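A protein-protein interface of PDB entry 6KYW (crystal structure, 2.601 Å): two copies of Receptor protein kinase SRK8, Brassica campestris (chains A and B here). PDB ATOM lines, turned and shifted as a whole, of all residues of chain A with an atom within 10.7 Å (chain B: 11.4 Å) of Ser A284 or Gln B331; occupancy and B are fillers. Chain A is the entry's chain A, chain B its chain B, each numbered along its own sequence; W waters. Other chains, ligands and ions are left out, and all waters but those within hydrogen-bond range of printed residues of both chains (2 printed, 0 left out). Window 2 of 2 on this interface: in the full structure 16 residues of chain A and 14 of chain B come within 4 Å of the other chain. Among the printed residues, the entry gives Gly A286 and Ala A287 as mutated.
The guanidinium group (NH1) of Arg B336 lies within hydrogen-bond range of the backbone carbonyl oxygen (O) of Phe A291 (2.9 Å).
The backbone NH (N) of Gln B331 lies within hydrogen-bond range of the side-chain amide oxygen (OD1) of Asn B329. N of Asn A289 lies within hydrogen-bond range of O of Thr A280, 2.8 Å away.
Among the printed residues, pairs that only touch across the chains: Ala A282 with Leu B335, Ser A284 with Gln B331, Ser A285 with Leu B335, Asn A289 with Leu B335, Phe A291 with Ala B334 and Phe A291 with Leu B335.
Ala A282 touches just one residue of chain B: Leu B335 (3.6 Å). No residue of chain B comes within 4 Å of Pro A283. Ser A284 touches one residue of chain B. Ser A285 touches just one residue of chain B: Leu B335 (3.8 Å). Of the printed residues of chain B, Asn A289 touches Leu B335 (3.2 Å). Printed residues of chain B within 4 Å of Phe A291: Ala B334, Leu B335 and Arg B336. No residue of chain A comes within 4 Å of Val B330. Of chain A, only Ser A284 (3.4 Å) comes within 4 Å of Gln B331. Of chain A, only Phe A291 comes within 4 Å of Ala B334. Of chain A, only Ala A282, Ser A285, Asn A289 and Phe A291 come within 4 Å of Leu B335. Printed residues of chain A within 4 Å of Arg B336: Phe A291 (2.9 Å). The nearest printed residue of chain B that does not touch Phe A291 is Trp B333 (6.1 Å).
Along chain A the printed residues that touch a printed residue of chain B span positions 282 to 291. Hydrophobic or aromatic side chains of chain B within 4 Å of the printed part of chain A: Leu B335.
No position is printed for both chains. Of the 7 pairs that touch across the chains among the printed residues, none has its exchanged pair printed and touching as well.
Water W2 lies within hydrogen-bond range of O of Arg B336 (2.6 Å) and O of Val A290 (3.1 Å). Water W1 bridges the backbone carbonyl oxygen of Phe A291 (2.8 Å) and the guanidinium group of Arg B336 (3.3 Å).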
ATOM      1  N   LEU A  78      30.464  -6.964  -9.232  1.00  0.00           N
ATOM      2  CA  LEU A  78      30.412  -8.174 -10.043  1.00  0.00           C
ATOM      3  C   LEU A  78      30.920  -9.350  -9.221  1.00  0.00           C
ATOM      4  O   LEU A  78      32.089  -9.373  -8.826  1.00  0.00           O
ATOM      5  CB  LEU A  78      31.231  -8.008 -11.328  1.00  0.00           C
ATOM      6  CG  LEU A  78      30.479  -7.640 -12.616  1.00  0.00           C
ATOM      7  CD1 LEU A  78      29.440  -6.549 -12.399  1.00  0.00           C
ATOM      8  CD2 LEU A  78      31.452  -7.223 -13.710  1.00  0.00           C
ATOM      9  N   TYR A 241      24.736   2.903 -26.336  1.00  0.00           N
ATOM     10  CA  TYR A 241      25.389   3.160 -25.059  1.00  0.00           C
ATOM     11  C   TYR A 241      26.888   3.441 -25.144  1.00  0.00           C
ATOM     12  O   TYR A 241      27.544   3.471 -24.094  1.00  0.00           O
ATOM     13  CB  TYR A 241      25.154   1.980 -24.114  1.00  0.00           C
ATOM     14  CG  TYR A 241      25.371   0.620 -24.733  1.00  0.00           C
ATOM     15  CD1 TYR A 241      24.410   0.042 -25.557  1.00  0.00           C
ATOM     16  CD2 TYR A 241      26.534  -0.098 -24.483  1.00  0.00           C
ATOM     17  CE1 TYR A 241      24.606  -1.214 -26.127  1.00  0.00           C
ATOM     18  CE2 TYR A 241      26.736  -1.361 -25.040  1.00  0.00           C
ATOM     19  CZ  TYR A 241      25.773  -1.910 -25.861  1.00  0.00           C
ATOM     20  OH  TYR A 241      25.976  -3.149 -26.411  1.00  0.00           O
ATOM     21  N   ASN A 261      25.549   5.376 -21.766  1.00  0.00           N
ATOM     22  CA  ASN A 261      24.588   5.054 -20.720  1.00  0.00           C
ATOM     23  C   ASN A 261      25.335   4.167 -19.729  1.00  0.00           C
ATOM     24  O   ASN A 261      25.854   3.106 -20.097  1.00  0.00           O
ATOM     25  CB  ASN A 261      23.336   4.379 -21.328  1.00  0.00           C
ATOM     26  CG  ASN A 261      22.387   3.734 -20.295  1.00  0.00           C
ATOM     27  OD1 ASN A 261      22.796   3.310 -19.212  1.00  0.00           O
ATOM     28  ND2 ASN A 261      21.094   3.656 -20.659  1.00  0.00           N
ATOM     29  N   SER A 263      24.481   2.415 -17.106  1.00  0.00           N
ATOM     30  CA  SER A 263      24.000   1.141 -16.583  1.00  0.00           C
ATOM     31  C   SER A 263      24.667  -0.032 -17.269  1.00  0.00           C
ATOM     32  O   SER A 263      24.415  -1.181 -16.893  1.00  0.00           O
ATOM     33  CB  SER A 263      22.477   1.025 -16.727  1.00  0.00           C
ATOM     34  OG  SER A 263      22.030   1.456 -18.002  1.00  0.00           O
ATOM     35  N   PHE A 264      25.496   0.246 -18.273  1.00  0.00           N
ATOM     36  CA  PHE A 264      26.241  -0.747 -19.029  1.00  0.00           C
ATOM     37  C   PHE A 264      27.704  -0.700 -18.636  1.00  0.00           C
ATOM     38  O   PHE A 264      28.278   0.385 -18.495  1.00  0.00           O
ATOM     39  CB  PHE A 264      26.172  -0.457 -20.518  1.00  0.00           C
ATOM     40  CG  PHE A 264      24.896  -0.822 -21.160  1.00  0.00           C
ATOM     41  CD1 PHE A 264      23.951   0.152 -21.433  1.00  0.00           C
ATOM     42  CD2 PHE A 264      24.657  -2.126 -21.555  1.00  0.00           C
ATOM     43  CE1 PHE A 264      22.765  -0.179 -22.074  1.00  0.00           C
ATOM     44  CE2 PHE A 264      23.481  -2.461 -22.197  1.00  0.00           C
ATOM     45  CZ  PHE A 264      22.536  -1.485 -22.460  1.00  0.00           C
ATOM     46  N   TYR A 265      28.313  -1.870 -18.509  1.00  0.00           N
ATOM     47  CA  TYR A 265      29.760  -2.009 -18.554  1.00  0.00           C
ATOM     48  C   TYR A 265      30.158  -2.562 -19.924  1.00  0.00           C
ATOM     49  O   TYR A 265      29.541  -3.523 -20.412  1.00  0.00           O
ATOM     50  CB  TYR A 265      30.263  -2.953 -17.462  1.00  0.00           C
ATOM     51  CG  TYR A 265      29.946  -2.547 -16.038  1.00  0.00           C
ATOM     52  CD1 TYR A 265      29.647  -1.227 -15.712  1.00  0.00           C
ATOM     53  CD2 TYR A 265      29.970  -3.491 -15.009  1.00  0.00           C
ATOM     54  CE1 TYR A 265      29.368  -0.860 -14.402  1.00  0.00           C
ATOM     55  CE2 TYR A 265      29.699  -3.132 -13.696  1.00  0.00           C
ATOM     56  CZ  TYR A 265      29.397  -1.816 -13.394  1.00  0.00           C
ATOM     57  OH  TYR A 265      29.126  -1.464 -12.081  1.00  0.00           O
ATOM     58  N   THR A 280      30.572  -6.944 -23.292  1.00  0.00           N
ATOM     59  CA  THR A 280      29.612  -6.021 -22.706  1.00  0.00           C
ATOM     60  C   THR A 280      28.809  -6.711 -21.604  1.00  0.00           C
ATOM     61  O   THR A 280      28.435  -7.887 -21.731  1.00  0.00           O
ATOM     62  CB  THR A 280      28.679  -5.460 -23.775  1.00  0.00           C
ATOM     63  OG1 THR A 280      29.449  -4.673 -24.684  1.00  0.00           O
ATOM     64  CG2 THR A 280      27.616  -4.578 -23.156  1.00  0.00           C
ATOM     65  N   TRP A 281      28.573  -5.973 -20.507  1.00  0.00           N
ATOM     66  CA  TRP A 281      27.725  -6.416 -19.398  1.00  0.00           C
ATOM     67  C   TRP A 281      26.462  -5.556 -19.361  1.00  0.00           C
ATOM     68  O   TRP A 281      26.519  -4.354 -19.070  1.00  0.00           O
ATOM     69  CB  TRP A 281      28.472  -6.337 -18.071  1.00  0.00           C
ATOM     70  CG  TRP A 281      27.638  -6.750 -16.893  1.00  0.00           C
ATOM     71  CD1 TRP A 281      26.524  -6.114 -16.387  1.00  0.00           C
ATOM     72  CD2 TRP A 281      27.863  -7.883 -16.056  1.00  0.00           C
ATOM     73  NE1 TRP A 281      26.049  -6.795 -15.296  1.00  0.00           N
ATOM     74  CE2 TRP A 281      26.853  -7.884 -15.071  1.00  0.00           C
ATOM     75  CE3 TRP A 281      28.819  -8.904 -16.047  1.00  0.00           C
ATOM     76  CZ2 TRP A 281      26.773  -8.866 -14.096  1.00  0.00           C
ATOM     77  CZ3 TRP A 281      28.739  -9.881 -15.072  1.00  0.00           C
ATOM     78  CH2 TRP A 281      27.724  -9.855 -14.110  1.00  0.00           C
ATOM     79  N   ALA A 282      25.376  -6.146 -19.620  1.00  0.00           N
ATOM     80  CA  ALA A 282      24.179  -5.332 -19.552  1.00  0.00           C
ATOM     81  C   ALA A 282      23.452  -5.577 -18.232  1.00  0.00           C
ATOM     82  O   ALA A 282      23.653  -6.623 -17.597  1.00  0.00           O
ATOM     83  CB  ALA A 282      23.250  -5.647 -20.730  1.00  0.00           C
ATOM     84  N   PRO A 283      22.625  -4.611 -17.788  1.00  0.00           N
ATOM     85  CA  PRO A 283      21.814  -4.838 -16.568  1.00  0.00           C
ATOM     86  C   PRO A 283      21.027  -6.140 -16.596  1.00  0.00           C
ATOM     87  O   PRO A 283      21.044  -6.904 -15.616  1.00  0.00           O
ATOM     88  CB  PRO A 283      20.887  -3.611 -16.536  1.00  0.00           C
ATOM     89  CG  PRO A 283      21.022  -2.939 -17.919  1.00  0.00           C
ATOM     90  CD  PRO A 283      22.422  -3.261 -18.351  1.00  0.00           C
ATOM     91  N   SER A 284      20.359  -6.422 -17.722  1.00  0.00           N
ATOM     92  CA  SER A 284      19.550  -7.623 -17.917  1.00  0.00           C
ATOM     93  C   SER A 284      20.223  -8.918 -17.482  1.00  0.00           C
ATOM     94  O   SER A 284      19.822  -9.521 -16.481  1.00  0.00           O
ATOM     95  CB  SER A 284      19.169  -7.765 -19.399  1.00  0.00           C
ATOM     96  N   SER A 285      21.235  -9.357 -18.224  1.00  0.00           N
ATOM     97  CA  SER A 285      21.927 -10.586 -17.868  1.00  0.00           C
ATOM     98  C   SER A 285      23.027 -10.317 -16.841  1.00  0.00           C
ATOM     99  O   SER A 285      23.441  -9.177 -16.595  1.00  0.00           O
ATOM    100  CB  SER A 285      22.523 -11.253 -19.107  1.00  0.00           C
ATOM    101  OG  SER A 285      22.949 -10.264 -20.029  1.00  0.00           O
ATOM    102  N   GLY A 286      23.496 -11.401 -16.238  1.00  0.00           N
ATOM    103  CA  GLY A 286      24.527 -11.312 -15.230  1.00  0.00           C
ATOM    104  C   GLY A 286      25.769 -11.989 -15.744  1.00  0.00           C
ATOM    105  O   GLY A 286      26.394 -12.798 -15.046  1.00  0.00           O
ATOM    106  N   ALA A 287      26.119 -11.677 -16.991  1.00  0.00           N
ATOM    107  CA  ALA A 287      27.343 -12.203 -17.562  1.00  0.00           C
ATOM    108  C   ALA A 287      27.927 -11.208 -18.550  1.00  0.00           C
ATOM    109  O   ALA A 287      27.242 -10.323 -19.078  1.00  0.00           O
ATOM    110  CB  ALA A 287      27.119 -13.552 -18.247  1.00  0.00           C
ATOM    111  N   TRP A 288      29.219 -11.372 -18.783  1.00  0.00           N
ATOM    112  CA  TRP A 288      29.887 -10.673 -19.859  1.00  0.00           C
ATOM    113  C   TRP A 288      29.527 -11.348 -21.173  1.00  0.00           C
ATOM    114  O   TRP A 288      29.607 -12.575 -21.286  1.00  0.00           O
ATOM    115  CB  TRP A 288      31.394 -10.701 -19.638  1.00  0.00           C
ATOM    116  CG  TRP A 288      31.886  -9.812 -18.528  1.00  0.00           C
ATOM    117  CD1 TRP A 288      32.380 -10.212 -17.312  1.00  0.00           C
ATOM    118  CD2 TRP A 288      31.976  -8.377 -18.548  1.00  0.00           C
ATOM    119  NE1 TRP A 288      32.750  -9.115 -16.571  1.00  0.00           N
ATOM    120  CE2 TRP A 288      32.520  -7.978 -17.307  1.00  0.00           C
ATOM    121  CE3 TRP A 288      31.670  -7.394 -19.504  1.00  0.00           C
ATOM    122  CZ2 TRP A 288      32.764  -6.639 -16.993  1.00  0.00           C
ATOM    123  CZ3 TRP A 288      31.898  -6.062 -19.191  1.00  0.00           C
ATOM    124  CH2 TRP A 288      32.434  -5.696 -17.939  1.00  0.00           C
ATOM    125  N   ASN A 289      29.131 -10.553 -22.160  1.00  0.00           N
ATOM    126  CA  ASN A 289      28.790 -11.068 -23.478  1.00  0.00           C
ATOM    127  C   ASN A 289      29.838 -10.645 -24.493  1.00  0.00           C
ATOM    128  O   ASN A 289      30.152  -9.453 -24.613  1.00  0.00           O
ATOM    129  CB  ASN A 289      27.407 -10.587 -23.919  1.00  0.00           C
ATOM    130  CG  ASN A 289      26.320 -11.299 -23.171  1.00  0.00           C
ATOM    131  OD1 ASN A 289      25.592 -10.696 -22.381  1.00  0.00           O
ATOM    132  ND2 ASN A 289      26.264 -12.626 -23.341  1.00  0.00           N
ATOM    133  N   VAL A 290      30.375 -11.621 -25.219  1.00  0.00           N
ATOM    134  CA  VAL A 290      31.312 -11.295 -26.281  1.00  0.00           C
ATOM    135  C   VAL A 290      30.502 -10.701 -27.425  1.00  0.00           C
ATOM    136  O   VAL A 290      29.800 -11.415 -28.148  1.00  0.00           O
ATOM    137  CB  VAL A 290      32.125 -12.513 -26.729  1.00  0.00           C
ATOM    138  CG1 VAL A 290      32.992 -12.144 -27.918  1.00  0.00           C
ATOM    139  CG2 VAL A 290      32.986 -13.039 -25.559  1.00  0.00           C
ATOM    140  N   PHE A 291      30.587  -9.383 -27.572  1.00  0.00           N
ATOM    141  CA  PHE A 291      29.886  -8.678 -28.637  1.00  0.00           C
ATOM    142  C   PHE A 291      30.596  -8.787 -29.987  1.00  0.00           C
ATOM    143  O   PHE A 291      29.935  -8.746 -31.024  1.00  0.00           O
ATOM    144  CB  PHE A 291      29.722  -7.207 -28.244  1.00  0.00           C
ATOM    145  CG  PHE A 291      28.619  -6.520 -28.960  1.00  0.00           C
ATOM    146  CD1 PHE A 291      27.299  -6.742 -28.597  1.00  0.00           C
ATOM    147  CD2 PHE A 291      28.890  -5.659 -29.997  1.00  0.00           C
ATOM    148  CE1 PHE A 291      26.277  -6.115 -29.269  1.00  0.00           C
ATOM    149  CE2 PHE A 291      27.864  -5.023 -30.676  1.00  0.00           C
ATOM    150  CZ  PHE A 291      26.559  -5.254 -30.318  1.00  0.00           C
ATOM    151  N   PRO B 317      24.834  -9.249 -37.498  1.00  0.00           N
ATOM    152  CA  PRO B 317      25.506 -10.435 -36.942  1.00  0.00           C
ATOM    153  C   PRO B 317      25.461 -11.626 -37.892  1.00  0.00           C
ATOM    154  O   PRO B 317      24.735 -11.603 -38.876  1.00  0.00           O
ATOM    155  CB  PRO B 317      24.702 -10.742 -35.673  1.00  0.00           C
ATOM    156  CG  PRO B 317      23.598  -9.669 -35.597  1.00  0.00           C
ATOM    157  CD  PRO B 317      23.469  -9.093 -36.967  1.00  0.00           C
ATOM    158  N   ASN B 326      11.242 -15.169 -35.768  1.00  0.00           N
ATOM    159  CA  ASN B 326      11.732 -14.025 -35.020  1.00  0.00           C
ATOM    160  C   ASN B 326      12.691 -14.527 -33.960  1.00  0.00           C
ATOM    161  O   ASN B 326      12.571 -15.672 -33.512  1.00  0.00           O
ATOM    162  CB  ASN B 326      10.583 -13.272 -34.319  1.00  0.00           C
ATOM    163  CG  ASN B 326       9.756 -12.427 -35.259  1.00  0.00           C
ATOM    164  OD1 ASN B 326      10.201 -12.036 -36.345  1.00  0.00           O
ATOM    165  ND2 ASN B 326       8.539 -12.113 -34.830  1.00  0.00           N
ATOM    166  N   PRO B 327      13.610 -13.678 -33.485  1.00  0.00           N
ATOM    167  CA  PRO B 327      14.514 -14.079 -32.393  1.00  0.00           C
ATOM    168  C   PRO B 327      13.766 -14.554 -31.150  1.00  0.00           C
ATOM    169  O   PRO B 327      12.853 -13.888 -30.659  1.00  0.00           O
ATOM    170  CB  PRO B 327      15.315 -12.798 -32.109  1.00  0.00           C
ATOM    171  CG  PRO B 327      15.249 -12.019 -33.334  1.00  0.00           C
ATOM    172  CD  PRO B 327      13.944 -12.344 -34.008  1.00  0.00           C
ATOM    173  N   GLY B 328      14.187 -15.703 -30.629  1.00  0.00           N
ATOM    174  CA  GLY B 328      13.510 -16.283 -29.483  1.00  0.00           C
ATOM    175  C   GLY B 328      13.621 -15.429 -28.235  1.00  0.00           C
ATOM    176  O   GLY B 328      12.645 -15.232 -27.510  1.00  0.00           O
ATOM    177  N   ASN B 329      14.812 -14.926 -27.957  1.00  0.00           N
ATOM    178  CA  ASN B 329      15.067 -14.114 -26.773  1.00  0.00           C
ATOM    179  C   ASN B 329      15.651 -12.800 -27.267  1.00  0.00           C
ATOM    180  O   ASN B 329      16.821 -12.739 -27.649  1.00  0.00           O
ATOM    181  CB  ASN B 329      15.997 -14.834 -25.813  1.00  0.00           C
ATOM    182  CG  ASN B 329      16.297 -14.026 -24.567  1.00  0.00           C
ATOM    183  OD1 ASN B 329      16.403 -12.782 -24.596  1.00  0.00           O
ATOM    184  ND2 ASN B 329      16.450 -14.736 -23.450  1.00  0.00           N
ATOM    185  N   VAL B 330      14.834 -11.749 -27.251  1.00  0.00           N
ATOM    186  CA  VAL B 330      15.195 -10.506 -27.921  1.00  0.00           C
ATOM    187  C   VAL B 330      16.300  -9.768 -27.167  1.00  0.00           C
ATOM    188  O   VAL B 330      17.137  -9.090 -27.780  1.00  0.00           O
ATOM    189  CB  VAL B 330      13.922  -9.663 -28.100  1.00  0.00           C
ATOM    190  CG1 VAL B 330      14.235  -8.186 -28.168  1.00  0.00           C
ATOM    191  CG2 VAL B 330      13.176 -10.120 -29.363  1.00  0.00           C
ATOM    192  N   GLN B 331      16.350  -9.903 -25.843  1.00  0.00           N
ATOM    193  CA  GLN B 331      17.400  -9.238 -25.085  1.00  0.00           C
ATOM    194  C   GLN B 331      18.741  -9.891 -25.355  1.00  0.00           C
ATOM    195  O   GLN B 331      19.744  -9.203 -25.562  1.00  0.00           O
ATOM    196  CB  GLN B 331      17.088  -9.281 -23.592  1.00  0.00           C
ATOM    197  CG  GLN B 331      16.411  -8.051 -23.067  1.00  0.00           C
ATOM    198  CD  GLN B 331      15.606  -8.350 -21.825  1.00  0.00           C
ATOM    199  OE1 GLN B 331      16.062  -8.127 -20.704  1.00  0.00           O
ATOM    200  NE2 GLN B 331      14.402  -8.878 -22.020  1.00  0.00           N
ATOM    201  N   GLN B 332      18.775 -11.225 -25.340  1.00  0.00           N
ATOM    202  CA  GLN B 332      20.002 -11.944 -25.658  1.00  0.00           C
ATOM    203  C   GLN B 332      20.489 -11.593 -27.060  1.00  0.00           C
ATOM    204  O   GLN B 332      21.675 -11.305 -27.261  1.00  0.00           O
ATOM    205  CB  GLN B 332      19.780 -13.443 -25.530  1.00  0.00           C
ATOM    206  CG  GLN B 332      19.655 -13.915 -24.106  1.00  0.00           C
ATOM    207  CD  GLN B 332      19.692 -15.432 -23.997  1.00  0.00           C
ATOM    208  OE1 GLN B 332      19.244 -16.148 -24.906  1.00  0.00           O
ATOM    209  NE2 GLN B 332      20.231 -15.934 -22.885  1.00  0.00           N
ATOM    210  N   TRP B 333      19.578 -11.576 -28.038  1.00  0.00           N
ATOM    211  CA  TRP B 333      19.991 -11.301 -29.409  1.00  0.00           C
ATOM    212  C   TRP B 333      20.546  -9.888 -29.554  1.00  0.00           C
ATOM    213  O   TRP B 333      21.428  -9.646 -30.387  1.00  0.00           O
ATOM    214  CB  TRP B 333      18.824 -11.502 -30.380  1.00  0.00           C
ATOM    215  CG  TRP B 333      18.736 -12.897 -30.989  1.00  0.00           C
ATOM    216  CD1 TRP B 333      18.496 -14.088 -30.321  1.00  0.00           C
ATOM    217  CD2 TRP B 333      18.865 -13.236 -32.378  1.00  0.00           C
ATOM    218  NE1 TRP B 333      18.478 -15.135 -31.220  1.00  0.00           N
ATOM    219  CE2 TRP B 333      18.701 -14.644 -32.485  1.00  0.00           C
ATOM    220  CE3 TRP B 333      19.112 -12.490 -33.542  1.00  0.00           C
ATOM    221  CZ2 TRP B 333      18.775 -15.324 -33.716  1.00  0.00           C
ATOM    222  CZ3 TRP B 333      19.182 -13.167 -34.769  1.00  0.00           C
ATOM    223  CH2 TRP B 333      19.011 -14.572 -34.844  1.00  0.00           C
ATOM    224  N   ALA B 334      20.043  -8.942 -28.769  1.00  0.00           N
ATOM    225  CA  ALA B 334      20.535  -7.578 -28.910  1.00  0.00           C
ATOM    226  C   ALA B 334      21.954  -7.459 -28.383  1.00  0.00           C
ATOM    227  O   ALA B 334      22.712  -6.591 -28.831  1.00  0.00           O
ATOM    228  CB  ALA B 334      19.608  -6.608 -28.197  1.00  0.00           C
ATOM    229  N   LEU B 335      22.333  -8.332 -27.454  1.00  0.00           N
ATOM    230  CA  LEU B 335      23.714  -8.467 -27.029  1.00  0.00           C
ATOM    231  C   LEU B 335      24.496  -9.455 -27.890  1.00  0.00           C
ATOM    232  O   LEU B 335      25.628  -9.807 -27.527  1.00  0.00           O
ATOM    233  CB  LEU B 335      23.763  -8.901 -25.564  1.00  0.00           C
ATOM    234  CG  LEU B 335      23.185  -7.926 -24.531  1.00  0.00           C
ATOM    235  CD1 LEU B 335      23.686  -8.296 -23.155  1.00  0.00           C
ATOM    236  CD2 LEU B 335      23.559  -6.480 -24.867  1.00  0.00           C
ATOM    237  N   ARG B 336      23.905  -9.922 -29.003  1.00  0.00           N
ATOM    238  CA  ARG B 336      24.512 -10.899 -29.913  1.00  0.00           C
ATOM    239  C   ARG B 336      24.774 -12.239 -29.242  1.00  0.00           C
ATOM    240  O   ARG B 336      25.677 -12.975 -29.641  1.00  0.00           O
ATOM    241  CB  ARG B 336      25.811 -10.375 -30.530  1.00  0.00           C
ATOM    242  CG  ARG B 336      25.575  -9.281 -31.486  1.00  0.00           C
ATOM    243  CD  ARG B 336      26.863  -8.678 -31.908  1.00  0.00           C
ATOM    244  NE  ARG B 336      26.656  -7.543 -32.796  1.00  0.00           N
ATOM    245  CZ  ARG B 336      27.636  -6.940 -33.459  1.00  0.00           C
ATOM    246  NH1 ARG B 336      28.891  -7.366 -33.326  1.00  0.00           N
ATOM    247  NH2 ARG B 336      27.370  -5.896 -34.234  1.00  0.00           N
ATOM    248  N   ASN B 337      24.020 -12.557 -28.201  1.00  0.00           N
ATOM    249  CA  ASN B 337      23.915 -13.932 -27.715  1.00  0.00           C
ATOM    250  C   ASN B 337      22.722 -14.562 -28.431  1.00  0.00           C
ATOM    251  O   ASN B 337      21.573 -14.273 -28.110  1.00  0.00           O
ATOM    252  CB  ASN B 337      23.738 -13.956 -26.206  1.00  0.00           C
ATOM    253  CG  ASN B 337      23.501 -15.342 -25.688  1.00  0.00           C
ATOM    254  OD1 ASN B 337      23.539 -16.316 -26.439  1.00  0.00           O
ATOM    255  ND2 ASN B 337      23.229 -15.443 -24.406  1.00  0.00           N
ATOM    256  N   GLN B 338      22.988 -15.404 -29.426  1.00  0.00           N
ATOM    257  CA  GLN B 338      21.943 -15.916 -30.301  1.00  0.00           C
ATOM    258  C   GLN B 338      21.645 -17.386 -30.071  1.00  0.00           C
ATOM    259  O   GLN B 338      21.056 -18.019 -30.946  1.00  0.00           O
ATOM    260  CB  GLN B 338      22.313 -15.708 -31.767  1.00  0.00           C
ATOM    261  CG  GLN B 338      22.338 -14.267 -32.187  1.00  0.00           C
ATOM    262  CD  GLN B 338      23.549 -13.928 -32.997  1.00  0.00           C
ATOM    263  OE1 GLN B 338      24.575 -14.597 -32.908  1.00  0.00           O
ATOM    264  NE2 GLN B 338      23.439 -12.893 -33.805  1.00  0.00           N
ATOM    265  N   ILE B 339      22.047 -17.952 -28.929  1.00  0.00           N
ATOM    266  CA  ILE B 339      21.760 -19.368 -28.697  1.00  0.00           C
ATOM    267  C   ILE B 339      20.256 -19.661 -28.728  1.00  0.00           C
ATOM    268  O   ILE B 339      19.848 -20.772 -29.073  1.00  0.00           O
ATOM    269  CB  ILE B 339      22.387 -19.840 -27.376  1.00  0.00           C
ATOM    270  CG1 ILE B 339      21.715 -19.180 -26.164  1.00  0.00           C
ATOM    271  CG2 ILE B 339      23.879 -19.596 -27.372  1.00  0.00           C
ATOM    272  CD1 ILE B 339      22.216 -19.791 -24.855  1.00  0.00           C
ATOM    273  N   SER B 340      19.414 -18.678 -28.398  1.00  0.00           N
ATOM    274  CA  SER B 340      17.966 -18.893 -28.388  1.00  0.00           C
ATOM    275  C   SER B 340      17.420 -19.252 -29.758  1.00  0.00           C
ATOM    276  O   SER B 340      16.303 -19.771 -29.853  1.00  0.00           O
ATOM    277  CB  SER B 340      17.223 -17.643 -27.905  1.00  0.00           C
ATOM    278  OG  SER B 340      17.175 -16.642 -28.942  1.00  0.00           O
ATOM    279  N   GLY B 341      18.156 -18.969 -30.822  1.00  0.00           N
ATOM    280  CA  GLY B 341      17.565 -19.271 -32.106  1.00  0.00           C
ATOM    281  C   GLY B 341      16.371 -18.364 -32.394  1.00  0.00           C
ATOM    282  O   GLY B 341      16.243 -17.257 -31.877  1.00  0.00           O
ATOM    283  N   LYS B 343      11.964 -18.286 -33.086  1.00  0.00           N
ATOM    284  CA  LYS B 343      10.648 -18.888 -32.921  1.00  0.00           C
ATOM    285  C   LYS B 343       9.774 -18.481 -34.104  1.00  0.00           C
ATOM    286  O   LYS B 343       9.963 -17.405 -34.687  1.00  0.00           O
ATOM    287  CB  LYS B 343      10.027 -18.438 -31.597  1.00  0.00           C
ATOM    288  CG  LYS B 343       9.216 -17.137 -31.731  1.00  0.00           C
ATOM    289  CD  LYS B 343       8.908 -16.409 -30.412  1.00  0.00           C
ATOM    290  CE  LYS B 343      10.033 -15.462 -29.961  1.00  0.00           C
ATOM    291  NZ  LYS B 343      10.043 -14.133 -30.669  1.00  0.00           N
HETATM  292  O   HOH W   1      29.980 -10.486 -33.196  1.00  0.00           O
HETATM  293  O   HOH W   2      28.250 -13.248 -30.154  1.00  0.00           O
